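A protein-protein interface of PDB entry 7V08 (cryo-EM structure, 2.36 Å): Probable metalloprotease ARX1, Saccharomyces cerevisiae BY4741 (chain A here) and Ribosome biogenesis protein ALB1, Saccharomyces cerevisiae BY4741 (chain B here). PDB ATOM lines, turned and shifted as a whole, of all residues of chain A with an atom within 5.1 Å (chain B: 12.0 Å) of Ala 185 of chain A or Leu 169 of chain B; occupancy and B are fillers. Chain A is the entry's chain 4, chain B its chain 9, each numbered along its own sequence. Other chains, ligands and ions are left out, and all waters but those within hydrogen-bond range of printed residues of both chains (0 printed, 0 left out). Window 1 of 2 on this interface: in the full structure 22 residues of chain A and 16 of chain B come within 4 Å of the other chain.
Of the 11 printed residues of chain B, 8 touch a printed residue of chain A.
Hydrophobic or aromatic side chains of chain B within 4 Å of the printed part of chain A: Leu 169, Pro 172 and Pro 175.
Hydrophobic or aromatic side chains of chain A within 4 Å of the printed part of chain B: Ala 185, His 188, Tyr 234, Trp 536 and Ile 537.
Among the printed residues, 15 pairs touch across the chains.
Among the printed residues, no Asp or Glu carboxylate lies within 4 Å of a Lys or Arg side-chain nitrogen of the other chain.
Ala 185 of chain A touches one residue of chain B.
Of chain A, only Ala 185 (3.7 Å), His 188 (3.9 Å), Ser 535 (2.9 Å), Trp 536 (3.3 Å) and Ile 537 (2.9 Å) come within 4 Å of Leu 169 of chain B.
No residue of chain B comes within 4 Å of Ala 181 of chain A.
No residue of chain B comes within 4 Å of Ala 183 of chain A.
No residue of chain B comes within 4 Å of Val 184 of chain A.
No residue of chain B comes within 4 Å of Ala 187 of chain A.
His 188 of chain A touches one residue of chain B.
Of chain B, only Thr 167 (3.2 Å) comes within 4 Å of Tyr 234 of chain A.
Ser 539 of chain A touches just these residues of chain B: Gly 166 (3.2 Å) and Thr 167 (3.0 Å).
Of the printed residues of chain A, Gly 171 of chain B touches Trp 536 (3.3 Å).
Printed residues of chain A within 4 Å of Gly 170 of chain B: Pro 534, Ser 535 and Trp 536.
Asp 182 of chain A touches none of the printed residues of chain B.
Gln 165 of chain B touches none of the printed residues of chain A.
The nearest residue of chain B that does not touch Ala 185 of chain A is Thr 167 of chain B (4.4 Å).
The backbone carbonyl oxygen of Thr 167 of chain B sits at hydrogen-bond distance from the backbone NH of Ser 539 of chain A.
N of Ile 537 of chain A is in hydrogen-bond range of O of Leu 169 of chain B.
O of Leu 169 of chain B sits close to O of Ser 535 of chain A, 2.9 Å away.
Among the printed residues, pairs that only touch across the chains: Ala 185 of chain A with Leu 169 of chain B (3.7 Å), His 188 of chain A with Leu 169 of chain B (3.9 Å), Tyr 234 of chain A with Thr 167 of chain B (3.2 Å), Pro 534 of chain A with Gly 170 of chain B (3.9 Å), Pro 534 of chain A with Pro 175 of chain B (3.8 Å), Ser 535 of chain A with Gly 170 of chain B (3.4 Å), Trp 536 of chain A with Leu 169 of chain B (3.3 Å), Trp 536 of chain A with Gly 170 of chain B (3.8 Å), Trp 536 of chain A with Gly 171 of chain B (3.3 Å), Trp 536 of chain A with Pro 172 of chain B (3.6 Å), Ile 537 of chain A with Thr 168 of chain B (3.5 Å) and Ser 539 of chain A with Gly 166 of chain B (3.2 Å).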
ATOM      1  N   LYS A 180     -14.324  25.080 -27.377  1.00  0.00           N
ATOM      2  CA  LYS A 180     -14.362  23.650 -27.663  1.00  0.00           C
ATOM      3  C   LYS A 180     -12.997  23.012 -27.443  1.00  0.00           C
ATOM      4  O   LYS A 180     -12.899  21.910 -26.886  1.00  0.00           O
ATOM      5  CB  LYS A 180     -14.853  23.422 -29.090  1.00  0.00           C
ATOM      6  CG  LYS A 180     -16.299  23.828 -29.285  1.00  0.00           C
ATOM      7  CD  LYS A 180     -16.757  23.701 -30.720  1.00  0.00           C
ATOM      8  CE  LYS A 180     -18.252  23.945 -30.808  1.00  0.00           C
ATOM      9  NZ  LYS A 180     -18.802  23.734 -32.170  1.00  0.00           N
ATOM     10  N   ALA A 181     -11.932  23.702 -27.862  1.00  0.00           N
ATOM     11  CA  ALA A 181     -10.579  23.227 -27.597  1.00  0.00           C
ATOM     12  C   ALA A 181     -10.292  23.188 -26.101  1.00  0.00           C
ATOM     13  O   ALA A 181      -9.690  22.227 -25.604  1.00  0.00           O
ATOM     14  CB  ALA A 181      -9.565  24.111 -28.322  1.00  0.00           C
ATOM     15  N   ASP A 182     -10.733  24.215 -25.367  1.00  0.00           N
ATOM     16  CA  ASP A 182     -10.559  24.226 -23.915  1.00  0.00           C
ATOM     17  C   ASP A 182     -11.235  23.019 -23.271  1.00  0.00           C
ATOM     18  O   ASP A 182     -10.651  22.352 -22.410  1.00  0.00           O
ATOM     19  CB  ASP A 182     -11.121  25.522 -23.323  1.00  0.00           C
ATOM     20  CG  ASP A 182     -10.458  26.764 -23.883  1.00  0.00           C
ATOM     21  OD1 ASP A 182      -9.270  26.703 -24.249  1.00  0.00           O
ATOM     22  OD2 ASP A 182     -11.134  27.811 -23.949  1.00  0.00           O
ATOM     23  N   ALA A 183     -12.466  22.718 -23.695  1.00  0.00           N
ATOM     24  CA  ALA A 183     -13.197  21.583 -23.135  1.00  0.00           C
ATOM     25  C   ALA A 183     -12.526  20.257 -23.472  1.00  0.00           C
ATOM     26  O   ALA A 183     -12.421  19.370 -22.612  1.00  0.00           O
ATOM     27  CB  ALA A 183     -14.642  21.592 -23.633  1.00  0.00           C
ATOM     28  N   VAL A 184     -12.068  20.099 -24.717  1.00  0.00           N
ATOM     29  CA  VAL A 184     -11.409  18.857 -25.116  1.00  0.00           C
ATOM     30  C   VAL A 184     -10.132  18.645 -24.311  1.00  0.00           C
ATOM     31  O   VAL A 184      -9.877  17.544 -23.800  1.00  0.00           O
ATOM     32  CB  VAL A 184     -11.137  18.857 -26.632  1.00  0.00           C
ATOM     33  CG1 VAL A 184     -10.149  17.760 -27.006  1.00  0.00           C
ATOM     34  CG2 VAL A 184     -12.432  18.664 -27.400  1.00  0.00           C
ATOM     35  N   ALA A 185      -9.322  19.699 -24.165  1.00  0.00           N
ATOM     36  CA  ALA A 185      -8.082  19.589 -23.402  1.00  0.00           C
ATOM     37  C   ALA A 185      -8.353  19.285 -21.936  1.00  0.00           C
ATOM     38  O   ALA A 185      -7.653  18.466 -21.325  1.00  0.00           O
ATOM     39  CB  ALA A 185      -7.267  20.875 -23.533  1.00  0.00           C
ATOM     40  N   ALA A 186      -9.357  19.945 -21.350  1.00  0.00           N
ATOM     41  CA  ALA A 186      -9.686  19.691 -19.953  1.00  0.00           C
ATOM     42  C   ALA A 186     -10.105  18.244 -19.745  1.00  0.00           C
ATOM     43  O   ALA A 186      -9.627  17.582 -18.814  1.00  0.00           O
ATOM     44  CB  ALA A 186     -10.794  20.639 -19.494  1.00  0.00           C
ATOM     45  N   ALA A 187     -10.970  17.729 -20.625  1.00  0.00           N
ATOM     46  CA  ALA A 187     -11.429  16.350 -20.500  1.00  0.00           C
ATOM     47  C   ALA A 187     -10.278  15.364 -20.648  1.00  0.00           C
ATOM     48  O   ALA A 187     -10.157  14.415 -19.860  1.00  0.00           O
ATOM     49  CB  ALA A 187     -12.516  16.067 -21.535  1.00  0.00           C
ATOM     50  N   HIS A 188      -9.402  15.589 -21.633  1.00  0.00           N
ATOM     51  CA  HIS A 188      -8.313  14.649 -21.879  1.00  0.00           C
ATOM     52  C   HIS A 188      -7.315  14.635 -20.726  1.00  0.00           C
ATOM     53  O   HIS A 188      -6.890  13.564 -20.268  1.00  0.00           O
ATOM     54  CB  HIS A 188      -7.613  14.993 -23.190  1.00  0.00           C
ATOM     55  CG  HIS A 188      -6.393  14.169 -23.449  1.00  0.00           C
ATOM     56  ND1 HIS A 188      -5.125  14.591 -23.116  1.00  0.00           N
ATOM     57  CD2 HIS A 188      -6.250  12.939 -23.993  1.00  0.00           C
ATOM     58  CE1 HIS A 188      -4.251  13.659 -23.451  1.00  0.00           C
ATOM     59  NE2 HIS A 188      -4.908  12.647 -23.986  1.00  0.00           N
ATOM     60  N   ILE A 189      -6.932  15.818 -20.240  1.00  0.00           N
ATOM     61  CA  ILE A 189      -5.960  15.895 -19.155  1.00  0.00           C
ATOM     62  C   ILE A 189      -6.547  15.334 -17.866  1.00  0.00           C
ATOM     63  O   ILE A 189      -5.850  14.658 -17.096  1.00  0.00           O
ATOM     64  CB  ILE A 189      -5.469  17.344 -18.996  1.00  0.00           C
ATOM     65  CG1 ILE A 189      -4.655  17.744 -20.223  1.00  0.00           C
ATOM     66  CG2 ILE A 189      -4.622  17.504 -17.752  1.00  0.00           C
ATOM     67  CD1 ILE A 189      -4.288  19.188 -20.262  1.00  0.00           C
ATOM     68  N   ALA A 190      -7.838  15.578 -17.615  1.00  0.00           N
ATOM     69  CA  ALA A 190      -8.478  14.994 -16.442  1.00  0.00           C
ATOM     70  C   ALA A 190      -8.507  13.473 -16.527  1.00  0.00           C
ATOM     71  O   ALA A 190      -8.267  12.788 -15.526  1.00  0.00           O
ATOM     72  CB  ALA A 190      -9.888  15.560 -16.281  1.00  0.00           C
ATOM     73  N   TYR A 234      -8.782  25.330 -17.131  1.00  0.00           N
ATOM     74  CA  TYR A 234      -9.181  25.451 -18.526  1.00  0.00           C
ATOM     75  C   TYR A 234     -10.484  26.219 -18.715  1.00  0.00           C
ATOM     76  O   TYR A 234     -11.004  26.251 -19.835  1.00  0.00           O
ATOM     77  CB  TYR A 234      -9.270  24.068 -19.171  1.00  0.00           C
ATOM     78  CG  TYR A 234      -7.921  23.574 -19.626  1.00  0.00           C
ATOM     79  CD1 TYR A 234      -7.382  24.001 -20.831  1.00  0.00           C
ATOM     80  CD2 TYR A 234      -7.170  22.718 -18.839  1.00  0.00           C
ATOM     81  CE1 TYR A 234      -6.147  23.574 -21.247  1.00  0.00           C
ATOM     82  CE2 TYR A 234      -5.928  22.282 -19.248  1.00  0.00           C
ATOM     83  CZ  TYR A 234      -5.421  22.716 -20.454  1.00  0.00           C
ATOM     84  OH  TYR A 234      -4.185  22.294 -20.877  1.00  0.00           O
ATOM     85  N   PRO A 534      -6.058  12.004 -29.239  1.00  0.00           N
ATOM     86  CA  PRO A 534      -6.681  13.330 -29.285  1.00  0.00           C
ATOM     87  C   PRO A 534      -6.582  13.966 -30.661  1.00  0.00           C
ATOM     88  O   PRO A 534      -5.654  13.707 -31.431  1.00  0.00           O
ATOM     89  CB  PRO A 534      -5.885  14.127 -28.248  1.00  0.00           C
ATOM     90  CG  PRO A 534      -4.554  13.477 -28.241  1.00  0.00           C
ATOM     91  CD  PRO A 534      -4.815  12.011 -28.450  1.00  0.00           C
ATOM     92  N   SER A 535      -7.563  14.812 -30.964  1.00  0.00           N
ATOM     93  CA  SER A 535      -7.573  15.575 -32.200  1.00  0.00           C
ATOM     94  C   SER A 535      -6.592  16.743 -32.097  1.00  0.00           C
ATOM     95  O   SER A 535      -5.943  16.958 -31.072  1.00  0.00           O
ATOM     96  CB  SER A 535      -8.986  16.066 -32.515  1.00  0.00           C
ATOM     97  OG  SER A 535      -9.841  14.995 -32.885  1.00  0.00           O
ATOM     98  N   TRP A 536      -6.479  17.505 -33.179  1.00  0.00           N
ATOM     99  CA  TRP A 536      -5.585  18.657 -33.230  1.00  0.00           C
ATOM    100  C   TRP A 536      -6.302  19.858 -32.629  1.00  0.00           C
ATOM    101  O   TRP A 536      -7.172  20.455 -33.263  1.00  0.00           O
ATOM    102  CB  TRP A 536      -5.158  18.939 -34.663  1.00  0.00           C
ATOM    103  CG  TRP A 536      -4.032  19.909 -34.771  1.00  0.00           C
ATOM    104  CD1 TRP A 536      -3.191  20.304 -33.773  1.00  0.00           C
ATOM    105  CD2 TRP A 536      -3.617  20.609 -35.946  1.00  0.00           C
ATOM    106  NE1 TRP A 536      -2.273  21.205 -34.256  1.00  0.00           N
ATOM    107  CE2 TRP A 536      -2.516  21.409 -35.589  1.00  0.00           C
ATOM    108  CE3 TRP A 536      -4.067  20.633 -37.271  1.00  0.00           C
ATOM    109  CZ2 TRP A 536      -1.863  22.228 -36.505  1.00  0.00           C
ATOM    110  CZ3 TRP A 536      -3.421  21.444 -38.172  1.00  0.00           C
ATOM    111  CH2 TRP A 536      -2.329  22.229 -37.790  1.00  0.00           C
ATOM    112  N   ILE A 537      -5.947  20.218 -31.397  1.00  0.00           N
ATOM    113  CA  ILE A 537      -6.538  21.373 -30.738  1.00  0.00           C
ATOM    114  C   ILE A 537      -5.418  22.270 -30.235  1.00  0.00           C
ATOM    115  O   ILE A 537      -4.270  21.849 -30.080  1.00  0.00           O
ATOM    116  CB  ILE A 537      -7.477  20.999 -29.569  1.00  0.00           C
ATOM    117  CG1 ILE A 537      -6.682  20.831 -28.274  1.00  0.00           C
ATOM    118  CG2 ILE A 537      -8.280  19.739 -29.869  1.00  0.00           C
ATOM    119  CD1 ILE A 537      -7.521  20.464 -27.114  1.00  0.00           C
ATOM    120  N   SER A 539      -5.239  25.499 -27.184  1.00  0.00           N
ATOM    121  CA  SER A 539      -5.938  26.272 -26.171  1.00  0.00           C
ATOM    122  C   SER A 539      -5.046  27.403 -25.687  1.00  0.00           C
ATOM    123  O   SER A 539      -3.818  27.307 -25.734  1.00  0.00           O
ATOM    124  CB  SER A 539      -6.360  25.390 -24.994  1.00  0.00           C
ATOM    125  OG  SER A 539      -7.043  26.140 -24.005  1.00  0.00           O
ATOM    126  N   GLN B 165       1.627  30.682 -23.458  1.00  0.00           N
ATOM    127  CA  GLN B 165       1.771  29.773 -24.589  1.00  0.00           C
ATOM    128  C   GLN B 165       0.517  28.937 -24.814  1.00  0.00           C
ATOM    129  O   GLN B 165       0.130  28.682 -25.952  1.00  0.00           O
ATOM    130  CB  GLN B 165       2.978  28.850 -24.392  1.00  0.00           C
ATOM    131  CG  GLN B 165       4.322  29.531 -24.601  1.00  0.00           C
ATOM    132  CD  GLN B 165       4.608  29.826 -26.060  1.00  0.00           C
ATOM    133  OE1 GLN B 165       3.880  29.384 -26.951  1.00  0.00           O
ATOM    134  NE2 GLN B 165       5.679  30.568 -26.313  1.00  0.00           N
ATOM    135  N   GLY B 166      -0.108  28.502 -23.725  1.00  0.00           N
ATOM    136  CA  GLY B 166      -1.315  27.703 -23.816  1.00  0.00           C
ATOM    137  C   GLY B 166      -1.024  26.219 -23.777  1.00  0.00           C
ATOM    138  O   GLY B 166      -0.195  25.769 -22.979  1.00  0.00           O
ATOM    139  N   THR B 167      -1.693  25.449 -24.634  1.00  0.00           N
ATOM    140  CA  THR B 167      -1.421  24.025 -24.756  1.00  0.00           C
ATOM    141  C   THR B 167      -1.821  23.550 -26.146  1.00  0.00           C
ATOM    142  O   THR B 167      -2.597  24.199 -26.852  1.00  0.00           O
ATOM    143  CB  THR B 167      -2.157  23.201 -23.693  1.00  0.00           C
ATOM    144  OG1 THR B 167      -1.792  21.821 -23.822  1.00  0.00           O
ATOM    145  CG2 THR B 167      -3.649  23.323 -23.872  1.00  0.00           C
ATOM    146  N   THR B 168      -1.279  22.398 -26.528  1.00  0.00           N
ATOM    147  CA  THR B 168      -1.580  21.797 -27.822  1.00  0.00           C
ATOM    148  C   THR B 168      -1.713  20.296 -27.633  1.00  0.00           C
ATOM    149  O   THR B 168      -0.925  19.690 -26.900  1.00  0.00           O
ATOM    150  CB  THR B 168      -0.489  22.114 -28.851  1.00  0.00           C
ATOM    151  OG1 THR B 168      -0.348  23.533 -28.983  1.00  0.00           O
ATOM    152  CG2 THR B 168      -0.834  21.519 -30.204  1.00  0.00           C
ATOM    153  N   LEU B 169      -2.725  19.708 -28.258  1.00  0.00           N
ATOM    154  CA  LEU B 169      -2.873  18.266 -28.338  1.00  0.00           C
ATOM    155  C   LEU B 169      -3.076  17.865 -29.791  1.00  0.00           C
ATOM    156  O   LEU B 169      -3.665  18.603 -30.585  1.00  0.00           O
ATOM    157  CB  LEU B 169      -4.044  17.781 -27.478  1.00  0.00           C
ATOM    158  CG  LEU B 169      -3.944  18.104 -25.991  1.00  0.00           C
ATOM    159  CD1 LEU B 169      -5.320  18.106 -25.374  1.00  0.00           C
ATOM    160  CD2 LEU B 169      -3.052  17.098 -25.287  1.00  0.00           C
ATOM    161  N   GLY B 170      -2.565  16.690 -30.139  1.00  0.00           N
ATOM    162  CA  GLY B 170      -2.700  16.205 -31.494  1.00  0.00           C
ATOM    163  C   GLY B 170      -1.827  16.962 -32.483  1.00  0.00           C
ATOM    164  O   GLY B 170      -0.904  17.692 -32.128  1.00  0.00           O
ATOM    165  N   GLY B 171      -2.152  16.772 -33.759  1.00  0.00           N
ATOM    166  CA  GLY B 171      -1.404  17.382 -34.830  1.00  0.00           C
ATOM    167  C   GLY B 171      -2.116  17.284 -36.164  1.00  0.00           C
ATOM    168  O   GLY B 171      -3.226  16.751 -36.265  1.00  0.00           O
ATOM    169  N   PRO B 172      -1.483  17.793 -37.221  1.00  0.00           N
ATOM    170  CA  PRO B 172      -2.123  17.820 -38.554  1.00  0.00           C
ATOM    171  C   PRO B 172      -2.191  16.445 -39.210  1.00  0.00           C
ATOM    172  O   PRO B 172      -1.556  16.159 -40.231  1.00  0.00           O
ATOM    173  CB  PRO B 172      -1.229  18.800 -39.322  1.00  0.00           C
ATOM    174  CG  PRO B 172       0.114  18.621 -38.705  1.00  0.00           C
ATOM    175  CD  PRO B 172      -0.146  18.413 -37.241  1.00  0.00           C
ATOM    176  N   PHE B 173      -2.986  15.562 -38.612  1.00  0.00           N
ATOM    177  CA  PHE B 173      -3.244  14.238 -39.160  1.00  0.00           C
ATOM    178  C   PHE B 173      -4.577  13.753 -38.610  1.00  0.00           C
ATOM    179  O   PHE B 173      -5.054  14.233 -37.579  1.00  0.00           O
ATOM    180  CB  PHE B 173      -2.109  13.255 -38.838  1.00  0.00           C
ATOM    181  CG  PHE B 173      -1.783  13.147 -37.375  1.00  0.00           C
ATOM    182  CD1 PHE B 173      -0.840  13.981 -36.796  1.00  0.00           C
ATOM    183  CD2 PHE B 173      -2.405  12.198 -36.581  1.00  0.00           C
ATOM    184  CE1 PHE B 173      -0.532  13.877 -35.449  1.00  0.00           C
ATOM    185  CE2 PHE B 173      -2.103  12.088 -35.236  1.00  0.00           C
ATOM    186  CZ  PHE B 173      -1.164  12.928 -34.669  1.00  0.00           C
ATOM    187  N   PHE B 174      -5.179  12.795 -39.311  1.00  0.00           N
ATOM    188  CA  PHE B 174      -6.494  12.306 -38.926  1.00  0.00           C
ATOM    189  C   PHE B 174      -6.340  11.029 -38.120  1.00  0.00           C
ATOM    190  O   PHE B 174      -5.923  10.005 -38.679  1.00  0.00           O
ATOM    191  CB  PHE B 174      -7.365  12.060 -40.157  1.00  0.00           C
ATOM    192  CG  PHE B 174      -7.829  13.318 -40.829  1.00  0.00           C
ATOM    193  CD1 PHE B 174      -8.537  14.269 -40.116  1.00  0.00           C
ATOM    194  CD2 PHE B 174      -7.563  13.547 -42.166  1.00  0.00           C
ATOM    195  CE1 PHE B 174      -8.969  15.419 -40.719  1.00  0.00           C
ATOM    196  CE2 PHE B 174      -7.992  14.707 -42.779  1.00  0.00           C
ATOM    197  CZ  PHE B 174      -8.696  15.643 -42.054  1.00  0.00           C
ATOM    198  N   PRO B 175      -6.653  11.032 -36.815  1.00  0.00           N
ATOM    199  CA  PRO B 175      -6.541   9.838 -35.973  1.00  0.00           C
ATOM    200  C   PRO B 175      -7.541   8.755 -36.367  1.00  0.00           C
ATOM    201  O   PRO B 175      -7.201   7.901 -37.186  1.00  0.00           O
ATOM    202  CB  PRO B 175      -6.843  10.368 -34.565  1.00  0.00           C
ATOM    203  CG  PRO B 175      -6.636  11.846 -34.653  1.00  0.00           C
ATOM    204  CD  PRO B 175      -7.056  12.211 -36.033  1.00  0.00           C
